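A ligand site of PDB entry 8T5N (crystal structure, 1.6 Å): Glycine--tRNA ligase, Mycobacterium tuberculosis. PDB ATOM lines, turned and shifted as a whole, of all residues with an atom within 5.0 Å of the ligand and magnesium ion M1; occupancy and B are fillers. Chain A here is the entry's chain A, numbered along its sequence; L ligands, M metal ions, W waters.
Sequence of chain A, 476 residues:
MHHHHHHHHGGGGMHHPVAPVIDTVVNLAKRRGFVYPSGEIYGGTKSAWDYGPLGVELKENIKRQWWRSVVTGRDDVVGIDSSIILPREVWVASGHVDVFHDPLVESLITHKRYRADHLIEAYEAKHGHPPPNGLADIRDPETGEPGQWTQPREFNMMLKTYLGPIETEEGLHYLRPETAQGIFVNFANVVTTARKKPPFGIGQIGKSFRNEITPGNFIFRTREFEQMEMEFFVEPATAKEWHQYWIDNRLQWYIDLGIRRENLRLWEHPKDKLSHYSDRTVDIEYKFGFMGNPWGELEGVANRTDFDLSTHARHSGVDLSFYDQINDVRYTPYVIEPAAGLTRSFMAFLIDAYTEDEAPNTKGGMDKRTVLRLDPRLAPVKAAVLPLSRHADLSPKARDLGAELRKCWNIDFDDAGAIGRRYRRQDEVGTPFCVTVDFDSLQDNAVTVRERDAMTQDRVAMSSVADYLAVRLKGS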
ATOM      1  N   GLU A 178      12.047  21.673  -6.369  1.00  0.00           N
ATOM      2  CA  GLU A 178      11.288  21.757  -7.613  1.00  0.00           C
ATOM      3  C   GLU A 178      12.100  21.068  -8.700  1.00  0.00           C
ATOM      4  O   GLU A 178      13.314  20.886  -8.581  1.00  0.00           O
ATOM      5  CB  GLU A 178      10.985  23.206  -8.013  1.00  0.00           C
ATOM      6  CG  GLU A 178      12.225  24.043  -8.230  1.00  0.00           C
ATOM      7  CD  GLU A 178      11.923  25.487  -8.530  1.00  0.00           C
ATOM      8  OE1 GLU A 178      10.800  25.944  -8.244  1.00  0.00           O
ATOM      9  OE2 GLU A 178      12.807  26.150  -9.065  1.00  0.00           O
ATOM     10  N   ARG A 210       9.709  19.190  -0.042  1.00  0.00           N
ATOM     11  CA  ARG A 210       9.710  20.447   0.713  1.00  0.00           C
ATOM     12  C   ARG A 210       9.348  20.170   2.152  1.00  0.00           C
ATOM     13  O   ARG A 210       8.410  19.407   2.418  1.00  0.00           O
ATOM     14  CB  ARG A 210       8.728  21.465   0.119  1.00  0.00           C
ATOM     15  CG  ARG A 210       9.052  21.888  -1.280  1.00  0.00           C
ATOM     16  CD  ARG A 210       8.049  22.883  -1.878  1.00  0.00           C
ATOM     17  NE  ARG A 210       8.417  23.131  -3.263  1.00  0.00           N
ATOM     18  CZ  ARG A 210       7.725  23.887  -4.108  1.00  0.00           C
ATOM     19  NH1 ARG A 210       6.666  24.581  -3.719  1.00  0.00           N
ATOM     20  NH2 ARG A 210       8.094  23.922  -5.380  1.00  0.00           N
ATOM     21  N   GLU A 212       7.469  21.231   4.359  1.00  0.00           N
ATOM     22  CA  GLU A 212       6.284  22.028   4.591  1.00  0.00           C
ATOM     23  C   GLU A 212       6.026  22.130   6.080  1.00  0.00           C
ATOM     24  O   GLU A 212       6.122  21.134   6.801  1.00  0.00           O
ATOM     25  CB  GLU A 212       5.075  21.425   3.885  1.00  0.00           C
ATOM     26  CG  GLU A 212       5.229  21.323   2.370  1.00  0.00           C
ATOM     27  CD  GLU A 212       5.089  22.667   1.672  1.00  0.00           C
ATOM     28  OE1 GLU A 212       4.694  23.646   2.345  1.00  0.00           O
ATOM     29  OE2 GLU A 212       5.366  22.759   0.464  1.00  0.00           O
ATOM     30  N   ILE A 219      -3.614  15.183  -0.164  1.00  0.00           N
ATOM     31  CA  ILE A 219      -2.394  15.233  -0.951  1.00  0.00           C
ATOM     32  C   ILE A 219      -2.170  16.592  -1.590  1.00  0.00           C
ATOM     33  O   ILE A 219      -1.291  16.739  -2.418  1.00  0.00           O
ATOM     34  CB  ILE A 219      -2.359  14.119  -2.013  1.00  0.00           C
ATOM     35  CG1 ILE A 219      -3.504  14.265  -3.014  1.00  0.00           C
ATOM     36  CG2 ILE A 219      -2.382  12.781  -1.323  1.00  0.00           C
ATOM     37  CD1 ILE A 219      -3.587  13.117  -4.053  1.00  0.00           C
ATOM     38  N   PHE A 220      -2.923  17.608  -1.177  1.00  0.00           N
ATOM     39  CA  PHE A 220      -2.772  18.942  -1.759  1.00  0.00           C
ATOM     40  C   PHE A 220      -1.395  19.536  -1.470  1.00  0.00           C
ATOM     41  O   PHE A 220      -0.767  20.127  -2.367  1.00  0.00           O
ATOM     42  CB  PHE A 220      -3.882  19.838  -1.198  1.00  0.00           C
ATOM     43  CG  PHE A 220      -3.763  21.274  -1.615  1.00  0.00           C
ATOM     44  CD1 PHE A 220      -4.214  21.694  -2.861  1.00  0.00           C
ATOM     45  CD2 PHE A 220      -3.204  22.210  -0.773  1.00  0.00           C
ATOM     46  CE1 PHE A 220      -4.108  23.028  -3.255  1.00  0.00           C
ATOM     47  CE2 PHE A 220      -3.076  23.537  -1.167  1.00  0.00           C
ATOM     48  CZ  PHE A 220      -3.522  23.942  -2.398  1.00  0.00           C
ATOM     49  N   ARG A 221      -0.951  19.436  -0.222  1.00  0.00           N
ATOM     50  CA  ARG A 221       0.345  20.013   0.196  1.00  0.00           C
ATOM     51  C   ARG A 221       1.109  18.993   1.044  1.00  0.00           C
ATOM     52  O   ARG A 221       0.854  18.916   2.240  1.00  0.00           O
ATOM     53  CB  ARG A 221       0.155  21.336   0.948  1.00  0.00           C
ATOM     54  CG  ARG A 221       1.433  22.071   1.311  1.00  0.00           C
ATOM     55  CD  ARG A 221       1.165  23.443   1.907  1.00  0.00           C
ATOM     56  NE  ARG A 221      -0.061  23.509   2.700  1.00  0.00           N
ATOM     57  CZ  ARG A 221      -1.174  24.122   2.326  1.00  0.00           C
ATOM     58  NH1 ARG A 221      -1.113  25.242   1.625  1.00  0.00           N
ATOM     59  NH2 ARG A 221      -2.354  23.614   2.639  1.00  0.00           N
ATOM     60  N   THR A 222       1.997  18.231   0.410  1.00  0.00           N
ATOM     61  CA  THR A 222       2.744  17.188   1.106  1.00  0.00           C
ATOM     62  C   THR A 222       4.241  17.475   1.050  1.00  0.00           C
ATOM     63  O   THR A 222       4.702  18.322   0.291  1.00  0.00           O
ATOM     64  CB  THR A 222       2.454  15.823   0.470  1.00  0.00           C
ATOM     65  OG1 THR A 222       2.821  15.816  -0.905  1.00  0.00           O
ATOM     66  CG2 THR A 222       0.945  15.528   0.554  1.00  0.00           C
ATOM     67  N   PHE A 225       6.166  15.029  -3.146  1.00  0.00           N
ATOM     68  CA  PHE A 225       5.122  15.198  -4.154  1.00  0.00           C
ATOM     69  C   PHE A 225       5.744  15.106  -5.528  1.00  0.00           C
ATOM     70  O   PHE A 225       6.959  15.003  -5.688  1.00  0.00           O
ATOM     71  CB  PHE A 225       4.340  16.528  -3.952  1.00  0.00           C
ATOM     72  CG  PHE A 225       5.203  17.769  -3.980  1.00  0.00           C
ATOM     73  CD1 PHE A 225       5.934  18.142  -2.869  1.00  0.00           C
ATOM     74  CD2 PHE A 225       5.245  18.574  -5.096  1.00  0.00           C
ATOM     75  CE1 PHE A 225       6.735  19.289  -2.876  1.00  0.00           C
ATOM     76  CE2 PHE A 225       6.039  19.733  -5.109  1.00  0.00           C
ATOM     77  CZ  PHE A 225       6.770  20.076  -4.003  1.00  0.00           C
ATOM     78  N   GLN A 227       5.643  16.872  -9.526  1.00  0.00           N
ATOM     79  CA  GLN A 227       5.327  18.030 -10.340  1.00  0.00           C
ATOM     80  C   GLN A 227       5.447  17.680 -11.799  1.00  0.00           C
ATOM     81  O   GLN A 227       6.148  16.734 -12.181  1.00  0.00           O
ATOM     82  CB  GLN A 227       6.276  19.212 -10.043  1.00  0.00           C
ATOM     83  CG  GLN A 227       6.220  19.678  -8.614  1.00  0.00           C
ATOM     84  CD  GLN A 227       7.124  20.827  -8.364  1.00  0.00           C
ATOM     85  OE1 GLN A 227       8.334  20.683  -8.433  1.00  0.00           O
ATOM     86  NE2 GLN A 227       6.539  21.985  -8.068  1.00  0.00           N
ATOM     87  N   GLU A 229       6.404  20.030 -14.916  1.00  0.00           N
ATOM     88  CA  GLU A 229       6.872  21.382 -15.180  1.00  0.00           C
ATOM     89  C   GLU A 229       7.464  21.464 -16.567  1.00  0.00           C
ATOM     90  O   GLU A 229       8.169  20.550 -17.023  1.00  0.00           O
ATOM     91  CB  GLU A 229       7.932  21.852 -14.165  1.00  0.00           C
ATOM     92  CG  GLU A 229       7.439  21.797 -12.715  1.00  0.00           C
ATOM     93  CD  GLU A 229       8.364  22.468 -11.725  1.00  0.00           C
ATOM     94  OE1 GLU A 229       9.451  21.901 -11.467  1.00  0.00           O
ATOM     95  OE2 GLU A 229       7.978  23.515 -11.162  1.00  0.00           O
ATOM     96  N   HIS A 269      -1.870  37.509 -10.696  1.00  0.00           N
ATOM     97  CA  HIS A 269      -1.171  38.118  -9.565  1.00  0.00           C
ATOM     98  C   HIS A 269      -1.052  39.634  -9.742  1.00  0.00           C
ATOM     99  O   HIS A 269      -0.572  40.098 -10.787  1.00  0.00           O
ATOM    100  CB  HIS A 269       0.234  37.562  -9.405  1.00  0.00           C
ATOM    101  CG  HIS A 269       0.285  36.150  -8.917  1.00  0.00           C
ATOM    102  ND1 HIS A 269       1.364  35.661  -8.193  1.00  0.00           N
ATOM    103  CD2 HIS A 269      -0.563  35.108  -9.078  1.00  0.00           C
ATOM    104  CE1 HIS A 269       1.162  34.379  -7.934  1.00  0.00           C
ATOM    105  NE2 HIS A 269       0.000  34.023  -8.453  1.00  0.00           N
ATOM    106  N   ASP A 283      -2.253  32.098 -11.934  1.00  0.00           N
ATOM    107  CA  ASP A 283      -2.501  30.777 -11.381  1.00  0.00           C
ATOM    108  C   ASP A 283      -3.832  30.242 -11.896  1.00  0.00           C
ATOM    109  O   ASP A 283      -4.836  30.959 -11.933  1.00  0.00           O
ATOM    110  CB  ASP A 283      -2.554  30.778  -9.838  1.00  0.00           C
ATOM    111  CG  ASP A 283      -1.229  31.118  -9.201  1.00  0.00           C
ATOM    112  OD1 ASP A 283      -0.197  30.991  -9.883  1.00  0.00           O
ATOM    113  OD2 ASP A 283      -1.228  31.519  -8.007  1.00  0.00           O
ATOM    114  N   GLU A 297      -4.563  26.906  -5.382  1.00  0.00           N
ATOM    115  CA  GLU A 297      -3.729  26.856  -6.565  1.00  0.00           C
ATOM    116  C   GLU A 297      -3.640  25.446  -7.104  1.00  0.00           C
ATOM    117  O   GLU A 297      -3.339  24.515  -6.353  1.00  0.00           O
ATOM    118  CB  GLU A 297      -2.316  27.371  -6.245  1.00  0.00           C
ATOM    119  CG  GLU A 297      -1.407  27.338  -7.455  1.00  0.00           C
ATOM    120  CD  GLU A 297       0.038  27.653  -7.090  1.00  0.00           C
ATOM    121  OE1 GLU A 297       0.269  28.549  -6.259  1.00  0.00           O
ATOM    122  OE2 GLU A 297       0.940  26.987  -7.647  1.00  0.00           O
ATOM    123  N   LEU A 298      -3.843  25.292  -8.399  1.00  0.00           N
ATOM    124  CA  LEU A 298      -3.646  24.016  -9.090  1.00  0.00           C
ATOM    125  C   LEU A 298      -2.394  24.009  -9.961  1.00  0.00           C
ATOM    126  O   LEU A 298      -1.662  23.023  -9.982  1.00  0.00           O
ATOM    127  CB  LEU A 298      -4.888  23.708  -9.927  1.00  0.00           C
ATOM    128  CG  LEU A 298      -4.940  22.394 -10.686  1.00  0.00           C
ATOM    129  CD1 LEU A 298      -4.760  21.167  -9.768  1.00  0.00           C
ATOM    130  CD2 LEU A 298      -6.279  22.273 -11.446  1.00  0.00           C
ATOM    131  N   GLU A 299      -2.122  25.111 -10.642  1.00  0.00           N
ATOM    132  CA  GLU A 299      -0.991  25.232 -11.552  1.00  0.00           C
ATOM    133  C   GLU A 299      -0.626  26.713 -11.645  1.00  0.00           C
ATOM    134  O   GLU A 299      -1.510  27.558 -11.700  1.00  0.00           O
ATOM    135  CB  GLU A 299      -1.329  24.661 -12.933  1.00  0.00           C
ATOM    136  CG  GLU A 299      -0.248  24.889 -13.987  1.00  0.00           C
ATOM    137  CD  GLU A 299      -0.430  24.100 -15.235  1.00  0.00           C
ATOM    138  OE1 GLU A 299      -1.393  23.312 -15.342  1.00  0.00           O
ATOM    139  OE2 GLU A 299       0.417  24.244 -16.150  1.00  0.00           O
ATOM    140  N   GLY A 300       0.663  27.023 -11.684  1.00  0.00           N
ATOM    141  CA  GLY A 300       1.128  28.402 -11.865  1.00  0.00           C
ATOM    142  C   GLY A 300       1.729  28.541 -13.253  1.00  0.00           C
ATOM    143  O   GLY A 300       2.476  27.669 -13.693  1.00  0.00           O
ATOM    144  N   ALA A 339       3.797  25.331 -14.471  1.00  0.00           N
ATOM    145  CA  ALA A 339       4.276  24.480 -13.363  1.00  0.00           C
ATOM    146  C   ALA A 339       3.056  23.839 -12.704  1.00  0.00           C
ATOM    147  O   ALA A 339       2.361  24.499 -11.925  1.00  0.00           O
ATOM    148  CB  ALA A 339       5.077  25.307 -12.374  1.00  0.00           C
ATOM    149  N   ALA A 340       2.814  22.578 -13.024  1.00  0.00           N
ATOM    150  CA  ALA A 340       1.665  21.825 -12.553  1.00  0.00           C
ATOM    151  C   ALA A 340       2.092  20.775 -11.527  1.00  0.00           C
ATOM    152  O   ALA A 340       3.275  20.503 -11.301  1.00  0.00           O
ATOM    153  CB  ALA A 340       0.940  21.154 -13.721  1.00  0.00           C
ATOM    154  N   GLY A 341       1.088  20.224 -10.867  1.00  0.00           N
ATOM    155  CA  GLY A 341       1.308  19.261  -9.824  1.00  0.00           C
ATOM    156  C   GLY A 341       0.608  17.966 -10.193  1.00  0.00           C
ATOM    157  O   GLY A 341      -0.617  17.943 -10.379  1.00  0.00           O
ATOM    158  N   THR A 343       0.437  15.109  -8.263  1.00  0.00           N
ATOM    159  CA  THR A 343      -0.372  14.595  -7.165  1.00  0.00           C
ATOM    160  C   THR A 343      -1.459  15.594  -6.763  1.00  0.00           C
ATOM    161  O   THR A 343      -2.563  15.186  -6.407  1.00  0.00           O
ATOM    162  CB  THR A 343       0.533  14.181  -6.012  1.00  0.00           C
ATOM    163  OG1 THR A 343       1.498  15.199  -5.768  1.00  0.00           O
ATOM    164  CG2 THR A 343       1.309  12.891  -6.377  1.00  0.00           C
ATOM    165  N   ARG A 344      -1.215  16.894  -6.903  1.00  0.00           N
ATOM    166  CA  ARG A 344      -2.306  17.840  -6.656  1.00  0.00           C
ATOM    167  C   ARG A 344      -3.415  17.704  -7.714  1.00  0.00           C
ATOM    168  O   ARG A 344      -4.600  17.753  -7.361  1.00  0.00           O
ATOM    169  CB  ARG A 344      -1.776  19.279  -6.600  1.00  0.00           C
ATOM    170  CG  ARG A 344      -2.802  20.238  -6.073  1.00  0.00           C
ATOM    171  CD  ARG A 344      -2.230  21.625  -5.798  1.00  0.00           C
ATOM    172  NE  ARG A 344      -1.348  21.700  -4.645  1.00  0.00           N
ATOM    173  CZ  ARG A 344      -0.785  22.806  -4.191  1.00  0.00           C
ATOM    174  NH1 ARG A 344      -0.986  23.979  -4.786  1.00  0.00           N
ATOM    175  NH2 ARG A 344       0.018  22.759  -3.116  1.00  0.00           N
HETATM  176  P1  LIG L   1       5.610  25.864  -7.254  1.00  0.00           P
HETATM  177  O1  LIG L   1       5.378  26.175  -5.821  1.00  0.00           O
HETATM  178  O2  LIG L   1       6.918  25.214  -7.585  1.00  0.00           O
HETATM  179  O3  LIG L   1       5.232  26.936  -8.273  1.00  0.00           O
HETATM  180  O4  LIG L   1       4.544  24.708  -7.520  1.00  0.00           O
HETATM  181  C1  LIG L   1       4.091  24.327  -8.802  1.00  0.00           C
HETATM  182  C2  LIG L   1       2.945  23.347  -8.626  1.00  0.00           C
HETATM  183  O5  LIG L   1       3.439  22.211  -7.867  1.00  0.00           O
HETATM  184  C3  LIG L   1       1.763  23.845  -7.809  1.00  0.00           C
HETATM  185  O6  LIG L   1       0.825  24.579  -8.587  1.00  0.00           O
HETATM  186  C4  LIG L   1       1.159  22.556  -7.255  1.00  0.00           C
HETATM  187  O7  LIG L   1       0.365  21.930  -8.260  1.00  0.00           O
HETATM  188  C5  LIG L   1       2.407  21.717  -7.032  1.00  0.00           C
HETATM  189  N1  LIG L   1       2.893  21.749  -5.637  1.00  0.00           N
HETATM  190  C6  LIG L   1       3.644  22.722  -5.057  1.00  0.00           C
HETATM  191  N2  LIG L   1       3.914  22.425  -3.769  1.00  0.00           N
HETATM  192  C7  LIG L   1       3.307  21.242  -3.502  1.00  0.00           C
HETATM  193  C8  LIG L   1       3.194  20.357  -2.347  1.00  0.00           C
HETATM  194  N3  LIG L   1       3.819  20.657  -1.200  1.00  0.00           N
HETATM  195  N4  LIG L   1       2.468  19.220  -2.473  1.00  0.00           N
HETATM  196  C9  LIG L   1       1.865  18.901  -3.628  1.00  0.00           C
HETATM  197  N5  LIG L   1       1.939  19.659  -4.730  1.00  0.00           N
HETATM  198  C10 LIG L   1       2.639  20.812  -4.726  1.00  0.00           C
HETATM  199 MG    MG M   1       2.354  29.945  -6.775  1.00  0.00          MG
HETATM  200 MG    MG M   2       9.253  27.055  -9.085  1.00  0.00          MG
HETATM  201  O   HOH W   1       3.773  31.633  -6.319  1.00  0.00           O
HETATM  202  O   HOH W   2       8.753  27.602  -7.113  1.00  0.00           O
HETATM  203  O   HOH W   3       2.338  30.679  -8.971  1.00  0.00           O
HETATM  204  O   HOH W   4       0.819  31.503  -6.222  1.00  0.00           O
HETATM  205  O   HOH W   5       4.473  24.258  -1.565  1.00  0.00           O
HETATM  206  O   HOH W   6       2.358  29.625  -4.630  1.00  0.00           O
HETATM  207  O   HOH W   7       1.464  18.025  -7.044  1.00  0.00           O
HETATM  208  O   HOH W   8       3.056  28.391  -8.131  1.00  0.00           O
HETATM  209  O   HOH W   9       3.005  26.566  -4.795  1.00  0.00           O
HETATM  210  O   HOH W  10       7.434  28.003 -10.226  1.00  0.00           O
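Of the 21 residues printed, 1 comes within 4 Å of magnesium ion M1.
N4 of the ligand lies close to O of Phe 220 (3.4 Å). Residues that only touch the ligand: Arg 221, Phe 225, Glu 299, Gly 300, Ala 339, Ala 340 and Arg 344. 15 residues have an atom within 4 Å of the ligand: Arg 210, Glu 212, Phe 220, Arg 221, Thr 222, Phe 225, Gln 227, Glu 297, Leu 298, Glu 299, Gly 300, Ala 339, Ala 340, Gly 341 and Arg 344.
The side-chain amide oxygen (OE1) of Gln 227 sits close to the side-chain carboxylate (OE1) of Glu 229, 3.5 Å away. The backbone carbonyl oxygen (O) of Glu 297 is in hydrogen-bond range of the guanidinium group (NH1) of Arg 344 (2.9 Å). The backbone carbonyl oxygen (O) of Phe 220 is in hydrogen-bond range of the guanidinium group (NE) of Arg 344, 2.8 Å away. The backbone carbonyl oxygen (O) of Gly 300 is in hydrogen-bond range of the backbone NH (N) of Ala 339.
Magnesium ion M1 is bound by water W6, 2.2 Å away. Magnesium ion M1 is bound by water W8 (2.2 Å). Water W1 is bound to magnesium ion M1, at 2.3 Å. Magnesium ion M1 is bound by water W4 (2.3 Å). Water W3 is bound to magnesium ion M1, at 2.3 Å. Magnesium ion M1 is bound by OE1 of Glu 297 (2.6 Å). Magnesium ion M1 has six donor atoms within binding distance.
O7 of the ligand sits at hydrogen-bond distance from N of Gly 341 (3.2 Å). The backbone NH (N) of Thr 222 lies within hydrogen-bond range of a nitrogen (N4) of the ligand. The backbone carbonyl oxygen (O) of Thr 222 lies within hydrogen-bond range of a nitrogen (N3) of the ligand (2.9 Å). OE2 of Glu 297 lies within hydrogen-bond range of O6 of the ligand, at 2.6 Å. O7 of the ligand is in hydrogen-bond range of O of Leu 298, at 2.9 Å. The guanidinium group (NH2) of Arg 210 lies within salt-bridge range of an oxygen (O2) of the ligand (2.8 Å). A nitrogen (N3) of the ligand lies within hydrogen-bond range of the side-chain carboxylate of Glu 212, at 3.1 Å. An oxygen (O5) of the ligand is in hydrogen-bond range of the side-chain amide nitrogen (NE2) of Gln 227 (3.1 Å).
Water W4 lies within hydrogen-bond range of OD2 of Asp 283 (2.7 Å) and NE2 of His 269 (3.5 Å). Water W8 bridges the side-chain carboxylate of Glu 297 (2.6 Å) and an oxygen (O3) of the ligand (2.6 Å). Water W7 lies within hydrogen-bond range of a nitrogen (N5) of the ligand, the backbone NH (N) of Arg 344 and the side-chain hydroxyl (OG1) of Thr 343. Water W5 lies within hydrogen-bond range of the side-chain carboxylate of Glu 212 (2.7 Å), a nitrogen (N2) of the ligand (2.9 Å) and the guanidinium group of Arg 210 (3.1 Å).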
